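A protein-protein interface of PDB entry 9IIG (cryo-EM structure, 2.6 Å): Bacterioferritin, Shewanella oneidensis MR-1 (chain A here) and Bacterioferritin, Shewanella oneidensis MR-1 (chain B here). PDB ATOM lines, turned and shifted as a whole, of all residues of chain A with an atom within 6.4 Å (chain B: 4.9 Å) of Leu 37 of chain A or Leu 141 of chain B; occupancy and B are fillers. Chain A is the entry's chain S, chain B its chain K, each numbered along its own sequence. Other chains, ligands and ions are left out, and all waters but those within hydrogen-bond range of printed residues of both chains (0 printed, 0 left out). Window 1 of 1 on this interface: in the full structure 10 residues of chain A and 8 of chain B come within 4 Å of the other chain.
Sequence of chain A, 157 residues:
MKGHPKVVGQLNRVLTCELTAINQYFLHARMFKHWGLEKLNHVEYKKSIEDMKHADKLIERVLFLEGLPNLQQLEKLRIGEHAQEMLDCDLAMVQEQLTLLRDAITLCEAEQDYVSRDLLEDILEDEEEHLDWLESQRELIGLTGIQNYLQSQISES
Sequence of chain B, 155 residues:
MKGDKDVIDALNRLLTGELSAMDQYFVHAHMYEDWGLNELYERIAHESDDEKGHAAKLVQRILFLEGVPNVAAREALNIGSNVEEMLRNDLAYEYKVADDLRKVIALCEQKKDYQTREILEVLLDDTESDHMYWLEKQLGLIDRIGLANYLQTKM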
ATOM      1  N   ALA A  29      13.765 -15.826  -9.516  1.00  0.00           N
ATOM      2  CA  ALA A  29      14.305 -17.158  -9.279  1.00  0.00           C
ATOM      3  C   ALA A  29      13.296 -18.230  -9.643  1.00  0.00           C
ATOM      4  O   ALA A  29      13.652 -19.266 -10.212  1.00  0.00           O
ATOM      5  CB  ALA A  29      14.723 -17.301  -7.820  1.00  0.00           C
ATOM      6  N   MET A  31      10.688 -17.858 -11.750  1.00  0.00           N
ATOM      7  CA  MET A  31      10.555 -17.833 -13.204  1.00  0.00           C
ATOM      8  C   MET A  31      11.698 -18.580 -13.876  1.00  0.00           C
ATOM      9  O   MET A  31      11.507 -19.201 -14.921  1.00  0.00           O
ATOM     10  CB  MET A  31      10.505 -16.392 -13.700  1.00  0.00           C
ATOM     11  CG  MET A  31       9.280 -15.619 -13.303  1.00  0.00           C
ATOM     12  SD  MET A  31       9.378 -13.921 -13.858  1.00  0.00           S
ATOM     13  CE  MET A  31       9.204 -14.143 -15.615  1.00  0.00           C
ATOM     14  N   PHE A  32      12.899 -18.517 -13.299  1.00  0.00           N
ATOM     15  CA  PHE A  32      14.027 -19.259 -13.855  1.00  0.00           C
ATOM     16  C   PHE A  32      13.860 -20.753 -13.635  1.00  0.00           C
ATOM     17  O   PHE A  32      14.132 -21.552 -14.534  1.00  0.00           O
ATOM     18  CB  PHE A  32      15.335 -18.777 -13.228  1.00  0.00           C
ATOM     19  CG  PHE A  32      15.842 -17.485 -13.793  1.00  0.00           C
ATOM     20  CD1 PHE A  32      15.746 -17.216 -15.141  1.00  0.00           C
ATOM     21  CD2 PHE A  32      16.406 -16.531 -12.967  1.00  0.00           C
ATOM     22  CE1 PHE A  32      16.208 -16.029 -15.655  1.00  0.00           C
ATOM     23  CE2 PHE A  32      16.861 -15.345 -13.475  1.00  0.00           C
ATOM     24  CZ  PHE A  32      16.764 -15.092 -14.820  1.00  0.00           C
ATOM     25  N   LYS A  33      13.441 -21.150 -12.434  1.00  0.00           N
ATOM     26  CA  LYS A  33      13.142 -22.555 -12.167  1.00  0.00           C
ATOM     27  C   LYS A  33      12.061 -23.085 -13.096  1.00  0.00           C
ATOM     28  O   LYS A  33      12.112 -24.241 -13.526  1.00  0.00           O
ATOM     29  CB  LYS A  33      12.706 -22.736 -10.717  1.00  0.00           C
ATOM     30  CG  LYS A  33      12.824 -24.154 -10.208  1.00  0.00           C
ATOM     31  CD  LYS A  33      12.014 -24.350  -8.941  1.00  0.00           C
ATOM     32  CE  LYS A  33      12.895 -24.720  -7.764  1.00  0.00           C
ATOM     33  NZ  LYS A  33      12.115 -25.012  -6.532  1.00  0.00           N
ATOM     34  N   HIS A  34      11.062 -22.260 -13.405  1.00  0.00           N
ATOM     35  CA  HIS A  34       9.985 -22.702 -14.274  1.00  0.00           C
ATOM     36  C   HIS A  34      10.474 -22.992 -15.682  1.00  0.00           C
ATOM     37  O   HIS A  34       9.880 -23.818 -16.386  1.00  0.00           O
ATOM     38  CB  HIS A  34       8.887 -21.641 -14.271  1.00  0.00           C
ATOM     39  CG  HIS A  34       7.757 -21.932 -15.201  1.00  0.00           C
ATOM     40  ND1 HIS A  34       6.914 -23.004 -15.020  1.00  0.00           N
ATOM     41  CD2 HIS A  34       7.298 -21.267 -16.283  1.00  0.00           C
ATOM     42  CE1 HIS A  34       6.004 -23.007 -15.974  1.00  0.00           C
ATOM     43  NE2 HIS A  34       6.212 -21.961 -16.749  1.00  0.00           N
ATOM     44  N   TRP A  35      11.557 -22.350 -16.103  1.00  0.00           N
ATOM     45  CA  TRP A  35      12.167 -22.544 -17.410  1.00  0.00           C
ATOM     46  C   TRP A  35      13.275 -23.579 -17.410  1.00  0.00           C
ATOM     47  O   TRP A  35      13.889 -23.798 -18.453  1.00  0.00           O
ATOM     48  CB  TRP A  35      12.724 -21.217 -17.908  1.00  0.00           C
ATOM     49  CG  TRP A  35      11.714 -20.168 -18.105  1.00  0.00           C
ATOM     50  CD1 TRP A  35      10.373 -20.327 -18.173  1.00  0.00           C
ATOM     51  CD2 TRP A  35      11.956 -18.764 -18.129  1.00  0.00           C
ATOM     52  NE1 TRP A  35       9.760 -19.111 -18.325  1.00  0.00           N
ATOM     53  CE2 TRP A  35      10.716 -18.132 -18.283  1.00  0.00           C
ATOM     54  CE3 TRP A  35      13.108 -17.983 -18.057  1.00  0.00           C
ATOM     55  CZ2 TRP A  35      10.595 -16.754 -18.370  1.00  0.00           C
ATOM     56  CZ3 TRP A  35      12.987 -16.629 -18.146  1.00  0.00           C
ATOM     57  CH2 TRP A  35      11.742 -16.023 -18.296  1.00  0.00           C
ATOM     58  N   GLY A  36      13.549 -24.219 -16.281  1.00  0.00           N
ATOM     59  CA  GLY A  36      14.604 -25.201 -16.208  1.00  0.00           C
ATOM     60  C   GLY A  36      15.994 -24.645 -16.080  1.00  0.00           C
ATOM     61  O   GLY A  36      16.955 -25.417 -16.105  1.00  0.00           O
ATOM     62  N   LEU A  37      16.143 -23.327 -15.986  1.00  0.00           N
ATOM     63  CA  LEU A  37      17.448 -22.713 -15.766  1.00  0.00           C
ATOM     64  C   LEU A  37      17.718 -22.761 -14.275  1.00  0.00           C
ATOM     65  O   LEU A  37      17.315 -21.873 -13.522  1.00  0.00           O
ATOM     66  CB  LEU A  37      17.477 -21.285 -16.298  1.00  0.00           C
ATOM     67  CG  LEU A  37      16.914 -21.106 -17.700  1.00  0.00           C
ATOM     68  CD1 LEU A  37      16.720 -19.652 -18.032  1.00  0.00           C
ATOM     69  CD2 LEU A  37      17.836 -21.751 -18.681  1.00  0.00           C
ATOM     70  N   GLU A  38      18.410 -23.807 -13.845  1.00  0.00           N
ATOM     71  CA  GLU A  38      18.521 -24.125 -12.429  1.00  0.00           C
ATOM     72  C   GLU A  38      19.619 -23.337 -11.745  1.00  0.00           C
ATOM     73  O   GLU A  38      19.487 -22.996 -10.568  1.00  0.00           O
ATOM     74  CB  GLU A  38      18.784 -25.615 -12.239  1.00  0.00           C
ATOM     75  CG  GLU A  38      17.590 -26.511 -12.494  1.00  0.00           C
ATOM     76  CD  GLU A  38      16.332 -26.039 -11.812  1.00  0.00           C
ATOM     77  OE1 GLU A  38      16.430 -25.490 -10.693  1.00  0.00           O
ATOM     78  OE2 GLU A  38      15.241 -26.213 -12.392  1.00  0.00           O
ATOM     79  N   LYS A  39      20.729 -23.069 -12.434  1.00  0.00           N
ATOM     80  CA  LYS A  39      21.807 -22.328 -11.790  1.00  0.00           C
ATOM     81  C   LYS A  39      21.422 -20.864 -11.614  1.00  0.00           C
ATOM     82  O   LYS A  39      21.796 -20.223 -10.624  1.00  0.00           O
ATOM     83  CB  LYS A  39      23.100 -22.491 -12.595  1.00  0.00           C
ATOM     84  CG  LYS A  39      24.306 -21.814 -11.974  1.00  0.00           C
ATOM     85  CD  LYS A  39      25.624 -22.111 -12.692  1.00  0.00           C
ATOM     86  CE  LYS A  39      25.770 -21.406 -14.023  1.00  0.00           C
ATOM     87  NZ  LYS A  39      27.116 -21.629 -14.630  1.00  0.00           N
ATOM     88  N   LEU A  40      20.609 -20.342 -12.531  1.00  0.00           N
ATOM     89  CA  LEU A  40      20.083 -18.992 -12.377  1.00  0.00           C
ATOM     90  C   LEU A  40      19.068 -18.928 -11.243  1.00  0.00           C
ATOM     91  O   LEU A  40      19.050 -17.965 -10.471  1.00  0.00           O
ATOM     92  CB  LEU A  40      19.455 -18.527 -13.684  1.00  0.00           C
ATOM     93  CG  LEU A  40      20.372 -17.809 -14.665  1.00  0.00           C
ATOM     94  CD1 LEU A  40      19.603 -17.351 -15.875  1.00  0.00           C
ATOM     95  CD2 LEU A  40      21.044 -16.651 -14.000  1.00  0.00           C
ATOM     96  N   ASN A  41      18.191 -19.929 -11.156  1.00  0.00           N
ATOM     97  CA  ASN A  41      17.382 -20.138  -9.962  1.00  0.00           C
ATOM     98  C   ASN A  41      18.211 -20.037  -8.697  1.00  0.00           C
ATOM     99  O   ASN A  41      17.862 -19.305  -7.772  1.00  0.00           O
ATOM    100  CB  ASN A  41      16.730 -21.511 -10.003  1.00  0.00           C
ATOM    101  CG  ASN A  41      15.755 -21.720  -8.877  1.00  0.00           C
ATOM    102  OD1 ASN A  41      15.523 -20.839  -8.062  1.00  0.00           O
ATOM    103  ND2 ASN A  41      15.279 -22.936  -8.750  1.00  0.00           N
ATOM    104  N   HIS A  42      19.276 -20.830  -8.613  1.00  0.00           N
ATOM    105  CA  HIS A  42      20.054 -20.899  -7.385  1.00  0.00           C
ATOM    106  C   HIS A  42      20.661 -19.548  -7.042  1.00  0.00           C
ATOM    107  O   HIS A  42      20.625 -19.119  -5.884  1.00  0.00           O
ATOM    108  CB  HIS A  42      21.142 -21.959  -7.528  1.00  0.00           C
ATOM    109  CG  HIS A  42      22.104 -22.001  -6.384  1.00  0.00           C
ATOM    110  ND1 HIS A  42      23.402 -21.548  -6.486  1.00  0.00           N
ATOM    111  CD2 HIS A  42      21.966 -22.460  -5.118  1.00  0.00           C
ATOM    112  CE1 HIS A  42      24.015 -21.712  -5.328  1.00  0.00           C
ATOM    113  NE2 HIS A  42      23.167 -22.265  -4.481  1.00  0.00           N
ATOM    114  N   ALA A  83      15.326 -14.030 -19.941  1.00  0.00           N
ATOM    115  CA  ALA A  83      16.489 -14.019 -19.060  1.00  0.00           C
ATOM    116  C   ALA A  83      17.241 -12.696 -19.119  1.00  0.00           C
ATOM    117  O   ALA A  83      17.573 -12.125 -18.077  1.00  0.00           O
ATOM    118  CB  ALA A  83      17.416 -15.180 -19.406  1.00  0.00           C
ATOM    119  N   LEU A 150      22.583 -19.498 -21.665  1.00  0.00           N
ATOM    120  CA  LEU A 150      21.448 -20.151 -21.034  1.00  0.00           C
ATOM    121  C   LEU A 150      21.669 -21.646 -20.892  1.00  0.00           C
ATOM    122  O   LEU A 150      21.163 -22.255 -19.949  1.00  0.00           O
ATOM    123  CB  LEU A 150      20.189 -19.867 -21.842  1.00  0.00           C
ATOM    124  CG  LEU A 150      19.609 -18.468 -21.662  1.00  0.00           C
ATOM    125  CD1 LEU A 150      18.276 -18.362 -22.340  1.00  0.00           C
ATOM    126  CD2 LEU A 150      19.492 -18.142 -20.195  1.00  0.00           C
ATOM    127  N   GLN A 151      22.421 -22.248 -21.809  1.00  0.00           N
ATOM    128  CA  GLN A 151      22.754 -23.659 -21.697  1.00  0.00           C
ATOM    129  C   GLN A 151      23.619 -23.932 -20.475  1.00  0.00           C
ATOM    130  O   GLN A 151      23.554 -25.018 -19.892  1.00  0.00           O
ATOM    131  CB  GLN A 151      23.459 -24.110 -22.969  1.00  0.00           C
ATOM    132  CG  GLN A 151      24.373 -25.278 -22.795  1.00  0.00           C
ATOM    133  CD  GLN A 151      24.711 -25.907 -24.095  1.00  0.00           C
ATOM    134  OE1 GLN A 151      24.843 -25.221 -25.097  1.00  0.00           O
ATOM    135  NE2 GLN A 151      24.872 -27.212 -24.099  1.00  0.00           N
ATOM    136  N   GLN A 153      23.261 -22.555 -17.638  1.00  0.00           N
ATOM    137  CA  GLN A 153      22.431 -22.391 -16.455  1.00  0.00           C
ATOM    138  C   GLN A 153      21.475 -23.551 -16.245  1.00  0.00           C
ATOM    139  O   GLN A 153      20.738 -23.553 -15.258  1.00  0.00           O
ATOM    140  CB  GLN A 153      21.637 -21.088 -16.548  1.00  0.00           C
ATOM    141  CG  GLN A 153      22.419 -19.892 -17.038  1.00  0.00           C
ATOM    142  CD  GLN A 153      23.615 -19.577 -16.172  1.00  0.00           C
ATOM    143  OE1 GLN A 153      23.530 -19.596 -14.953  1.00  0.00           O
ATOM    144  NE2 GLN A 153      24.735 -19.269 -16.802  1.00  0.00           N
ATOM    145  N   ILE A 154      21.467 -24.529 -17.146  1.00  0.00           N
ATOM    146  CA  ILE A 154      20.533 -25.644 -17.042  1.00  0.00           C
ATOM    147  C   ILE A 154      20.796 -26.457 -15.781  1.00  0.00           C
ATOM    148  O   ILE A 154      19.867 -26.822 -15.055  1.00  0.00           O
ATOM    149  CB  ILE A 154      20.611 -26.518 -18.307  1.00  0.00           C
ATOM    150  CG1 ILE A 154      20.052 -25.770 -19.511  1.00  0.00           C
ATOM    151  CG2 ILE A 154      19.889 -27.823 -18.104  1.00  0.00           C
ATOM    152  CD1 ILE A 154      19.944 -26.613 -20.740  1.00  0.00           C
ATOM    153  N   SER A 155      22.058 -26.749 -15.497  1.00  0.00           N
ATOM    154  CA  SER A 155      22.421 -27.557 -14.344  1.00  0.00           C
ATOM    155  C   SER A 155      22.844 -26.648 -13.201  1.00  0.00           C
ATOM    156  O   SER A 155      23.631 -25.716 -13.397  1.00  0.00           O
ATOM    157  CB  SER A 155      23.546 -28.531 -14.690  1.00  0.00           C
ATOM    158  OG  SER A 155      23.078 -29.559 -15.540  1.00  0.00           O
ATOM    159  N   LYS B 137       9.187 -27.929 -19.171  1.00  0.00           N
ATOM    160  CA  LYS B 137      10.470 -27.255 -18.997  1.00  0.00           C
ATOM    161  C   LYS B 137      11.438 -27.623 -20.110  1.00  0.00           C
ATOM    162  O   LYS B 137      12.168 -26.765 -20.614  1.00  0.00           O
ATOM    163  CB  LYS B 137      11.065 -27.610 -17.638  1.00  0.00           C
ATOM    164  CG  LYS B 137      10.345 -26.990 -16.463  1.00  0.00           C
ATOM    165  CD  LYS B 137      11.145 -27.160 -15.197  1.00  0.00           C
ATOM    166  CE  LYS B 137      11.209 -28.617 -14.814  1.00  0.00           C
ATOM    167  NZ  LYS B 137      11.891 -28.849 -13.522  1.00  0.00           N
ATOM    168  N   GLN B 138      11.467 -28.898 -20.501  1.00  0.00           N
ATOM    169  CA  GLN B 138      12.390 -29.343 -21.540  1.00  0.00           C
ATOM    170  C   GLN B 138      12.051 -28.719 -22.880  1.00  0.00           C
ATOM    171  O   GLN B 138      12.945 -28.314 -23.630  1.00  0.00           O
ATOM    172  CB  GLN B 138      12.362 -30.863 -21.664  1.00  0.00           C
ATOM    173  CG  GLN B 138      12.874 -31.596 -20.465  1.00  0.00           C
ATOM    174  CD  GLN B 138      13.881 -30.808 -19.681  1.00  0.00           C
ATOM    175  OE1 GLN B 138      15.026 -30.672 -20.085  1.00  0.00           O
ATOM    176  NE2 GLN B 138      13.462 -30.290 -18.539  1.00  0.00           N
ATOM    177  N   LEU B 139      10.768 -28.647 -23.207  1.00  0.00           N
ATOM    178  CA  LEU B 139      10.379 -28.043 -24.472  1.00  0.00           C
ATOM    179  C   LEU B 139      10.646 -26.542 -24.464  1.00  0.00           C
ATOM    180  O   LEU B 139      11.074 -25.974 -25.476  1.00  0.00           O
ATOM    181  CB  LEU B 139       8.914 -28.365 -24.757  1.00  0.00           C
ATOM    182  CG  LEU B 139       8.688 -29.879 -24.921  1.00  0.00           C
ATOM    183  CD1 LEU B 139       7.238 -30.212 -25.191  1.00  0.00           C
ATOM    184  CD2 LEU B 139       9.566 -30.451 -26.024  1.00  0.00           C
ATOM    185  N   GLY B 140      10.467 -25.894 -23.313  1.00  0.00           N
ATOM    186  CA  GLY B 140      10.831 -24.490 -23.213  1.00  0.00           C
ATOM    187  C   GLY B 140      12.325 -24.257 -23.333  1.00  0.00           C
ATOM    188  O   GLY B 140      12.762 -23.271 -23.925  1.00  0.00           O
ATOM    189  N   LEU B 141      13.130 -25.165 -22.781  1.00  0.00           N
ATOM    190  CA  LEU B 141      14.575 -25.056 -22.941  1.00  0.00           C
ATOM    191  C   LEU B 141      14.988 -25.258 -24.389  1.00  0.00           C
ATOM    192  O   LEU B 141      15.867 -24.555 -24.885  1.00  0.00           O
ATOM    193  CB  LEU B 141      15.300 -26.056 -22.048  1.00  0.00           C
ATOM    194  CG  LEU B 141      15.345 -25.735 -20.561  1.00  0.00           C
ATOM    195  CD1 LEU B 141      15.731 -26.958 -19.770  1.00  0.00           C
ATOM    196  CD2 LEU B 141      16.302 -24.600 -20.304  1.00  0.00           C
ATOM    197  N   ILE B 142      14.385 -26.226 -25.076  1.00  0.00           N
ATOM    198  CA  ILE B 142      14.657 -26.377 -26.503  1.00  0.00           C
ATOM    199  C   ILE B 142      14.329 -25.085 -27.231  1.00  0.00           C
ATOM    200  O   ILE B 142      15.046 -24.668 -28.146  1.00  0.00           O
ATOM    201  CB  ILE B 142      13.869 -27.564 -27.083  1.00  0.00           C
ATOM    202  CG1 ILE B 142      14.443 -28.878 -26.583  1.00  0.00           C
ATOM    203  CG2 ILE B 142      13.916 -27.537 -28.590  1.00  0.00           C
ATOM    204  CD1 ILE B 142      13.547 -30.052 -26.802  1.00  0.00           C
ATOM    205  N   ASP B 143      13.247 -24.422 -26.827  1.00  0.00           N
ATOM    206  CA  ASP B 143      12.884 -23.161 -27.462  1.00  0.00           C
ATOM    207  C   ASP B 143      13.878 -22.050 -27.139  1.00  0.00           C
ATOM    208  O   ASP B 143      14.096 -21.153 -27.958  1.00  0.00           O
ATOM    209  CB  ASP B 143      11.475 -22.758 -27.040  1.00  0.00           C
ATOM    210  CG  ASP B 143      10.412 -23.682 -27.595  1.00  0.00           C
ATOM    211  OD1 ASP B 143      10.758 -24.791 -28.055  1.00  0.00           O
ATOM    212  OD2 ASP B 143       9.224 -23.297 -27.570  1.00  0.00           O
ATOM    213  N   ARG B 144      14.480 -22.081 -25.951  1.00  0.00           N
ATOM    214  CA  ARG B 144      15.360 -20.986 -25.545  1.00  0.00           C
ATOM    215  C   ARG B 144      16.781 -21.157 -26.068  1.00  0.00           C
ATOM    216  O   ARG B 144      17.314 -20.251 -26.713  1.00  0.00           O
ATOM    217  CB  ARG B 144      15.362 -20.838 -24.024  1.00  0.00           C
ATOM    218  CG  ARG B 144      14.029 -20.381 -23.512  1.00  0.00           C
ATOM    219  CD  ARG B 144      13.952 -20.178 -22.021  1.00  0.00           C
ATOM    220  NE  ARG B 144      12.575 -19.845 -21.675  1.00  0.00           N
ATOM    221  CZ  ARG B 144      12.076 -18.616 -21.666  1.00  0.00           C
ATOM    222  NH1 ARG B 144      12.838 -17.556 -21.877  1.00  0.00           N
ATOM    223  NH2 ARG B 144      10.777 -18.447 -21.447  1.00  0.00           N
ATOM    224  N   ILE B 145      17.417 -22.299 -25.802  1.00  0.00           N
ATOM    225  CA  ILE B 145      18.811 -22.495 -26.182  1.00  0.00           C
ATOM    226  C   ILE B 145      18.969 -23.114 -27.557  1.00  0.00           C
ATOM    227  O   ILE B 145      20.082 -23.094 -28.102  1.00  0.00           O
ATOM    228  CB  ILE B 145      19.573 -23.355 -25.156  1.00  0.00           C
ATOM    229  CG1 ILE B 145      18.867 -24.671 -24.912  1.00  0.00           C
ATOM    230  CG2 ILE B 145      19.637 -22.636 -23.852  1.00  0.00           C
ATOM    231  CD1 ILE B 145      19.574 -25.533 -23.929  1.00  0.00           C
ATOM    232  N   GLY B 146      17.915 -23.667 -28.130  1.00  0.00           N
ATOM    233  CA  GLY B 146      18.021 -24.395 -29.373  1.00  0.00           C
ATOM    234  C   GLY B 146      18.154 -25.888 -29.144  1.00  0.00           C
ATOM    235  O   GLY B 146      18.466 -26.358 -28.053  1.00  0.00           O
ATOM    236  N   TYR B 150      20.432 -27.934 -26.492  1.00  0.00           N
ATOM    237  CA  TYR B 150      19.659 -28.726 -25.547  1.00  0.00           C
ATOM    238  C   TYR B 150      20.148 -30.160 -25.526  1.00  0.00           C
ATOM    239  O   TYR B 150      20.321 -30.754 -24.459  1.00  0.00           O
ATOM    240  CB  TYR B 150      18.170 -28.682 -25.884  1.00  0.00           C
ATOM    241  CG  TYR B 150      17.383 -29.657 -25.044  1.00  0.00           C
ATOM    242  CD1 TYR B 150      17.053 -29.350 -23.737  1.00  0.00           C
ATOM    243  CD2 TYR B 150      17.010 -30.898 -25.538  1.00  0.00           C
ATOM    244  CE1 TYR B 150      16.366 -30.232 -22.962  1.00  0.00           C
ATOM    245  CE2 TYR B 150      16.322 -31.784 -24.760  1.00  0.00           C
ATOM    246  CZ  TYR B 150      16.003 -31.447 -23.475  1.00  0.00           C
ATOM    247  OH  TYR B 150      15.312 -32.329 -22.691  1.00  0.00           O
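Printed residues of chain B within 4 Å of Leu 37 of chain A: Leu 141 (3.6 Å).
Lys 39 of chain A touches none of the printed residues of chain B.
His 42 of chain A touches none of the printed residues of chain B.
Printed residues of chain B within 4 Å of Leu 150 of chain A: Ile 145.
Printed residues of chain B within 4 Å of Ile 154 of chain A: Ile 145.
Printed residues of chain A within 4 Å of Leu 141 of chain B: Trp 35 (3.1 Å) and Leu 37 (3.6 Å).
The nearest printed residue of chain B that does not touch Gln 151 of chain A is Tyr 150 of chain B (5.1 Å).
The backbone carbonyl oxygen (O) of Phe 32 of chain A lies within hydrogen-bond range of the backbone NH (N) of Leu 37 of chain A.
Of the 11 printed residues of chain B, 4 touch a printed residue of chain A.
Hydrophobic or aromatic side chains of chain B that line the printed part of chain A: Leu 141 and Ile 145.
Along chain B the printed residues that touch a printed residue of chain A span positions 137 to 145.
Along chain A the printed residues that touch a printed residue of chain B span positions 33 to 154.
Among the printed residues, 9 pairs touch across the chains.
Among the printed residues, pairs that only touch across the chains: Trp 35 of chain A with Leu 141 of chain B (3.1 Å), His 34 of chain A with Lys 137 of chain B (3.2 Å), Ile 154 of chain A with Ile 145 of chain B (3.4 Å), Leu 150 of chain A with Ile 145 of chain B (3.5 Å), Gln 151 of chain A with Ile 145 of chain B (3.5 Å), Lys 33 of chain A with Lys 137 of chain B (3.5 Å), Leu 37 of chain A with Leu 141 of chain B (3.6 Å) and Gly 36 of chain A with Lys 137 of chain B (3.95 Å).
NH2 of Arg 144 of chain B sits close to NE1 of Trp 35 of chain A (3.3 Å).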
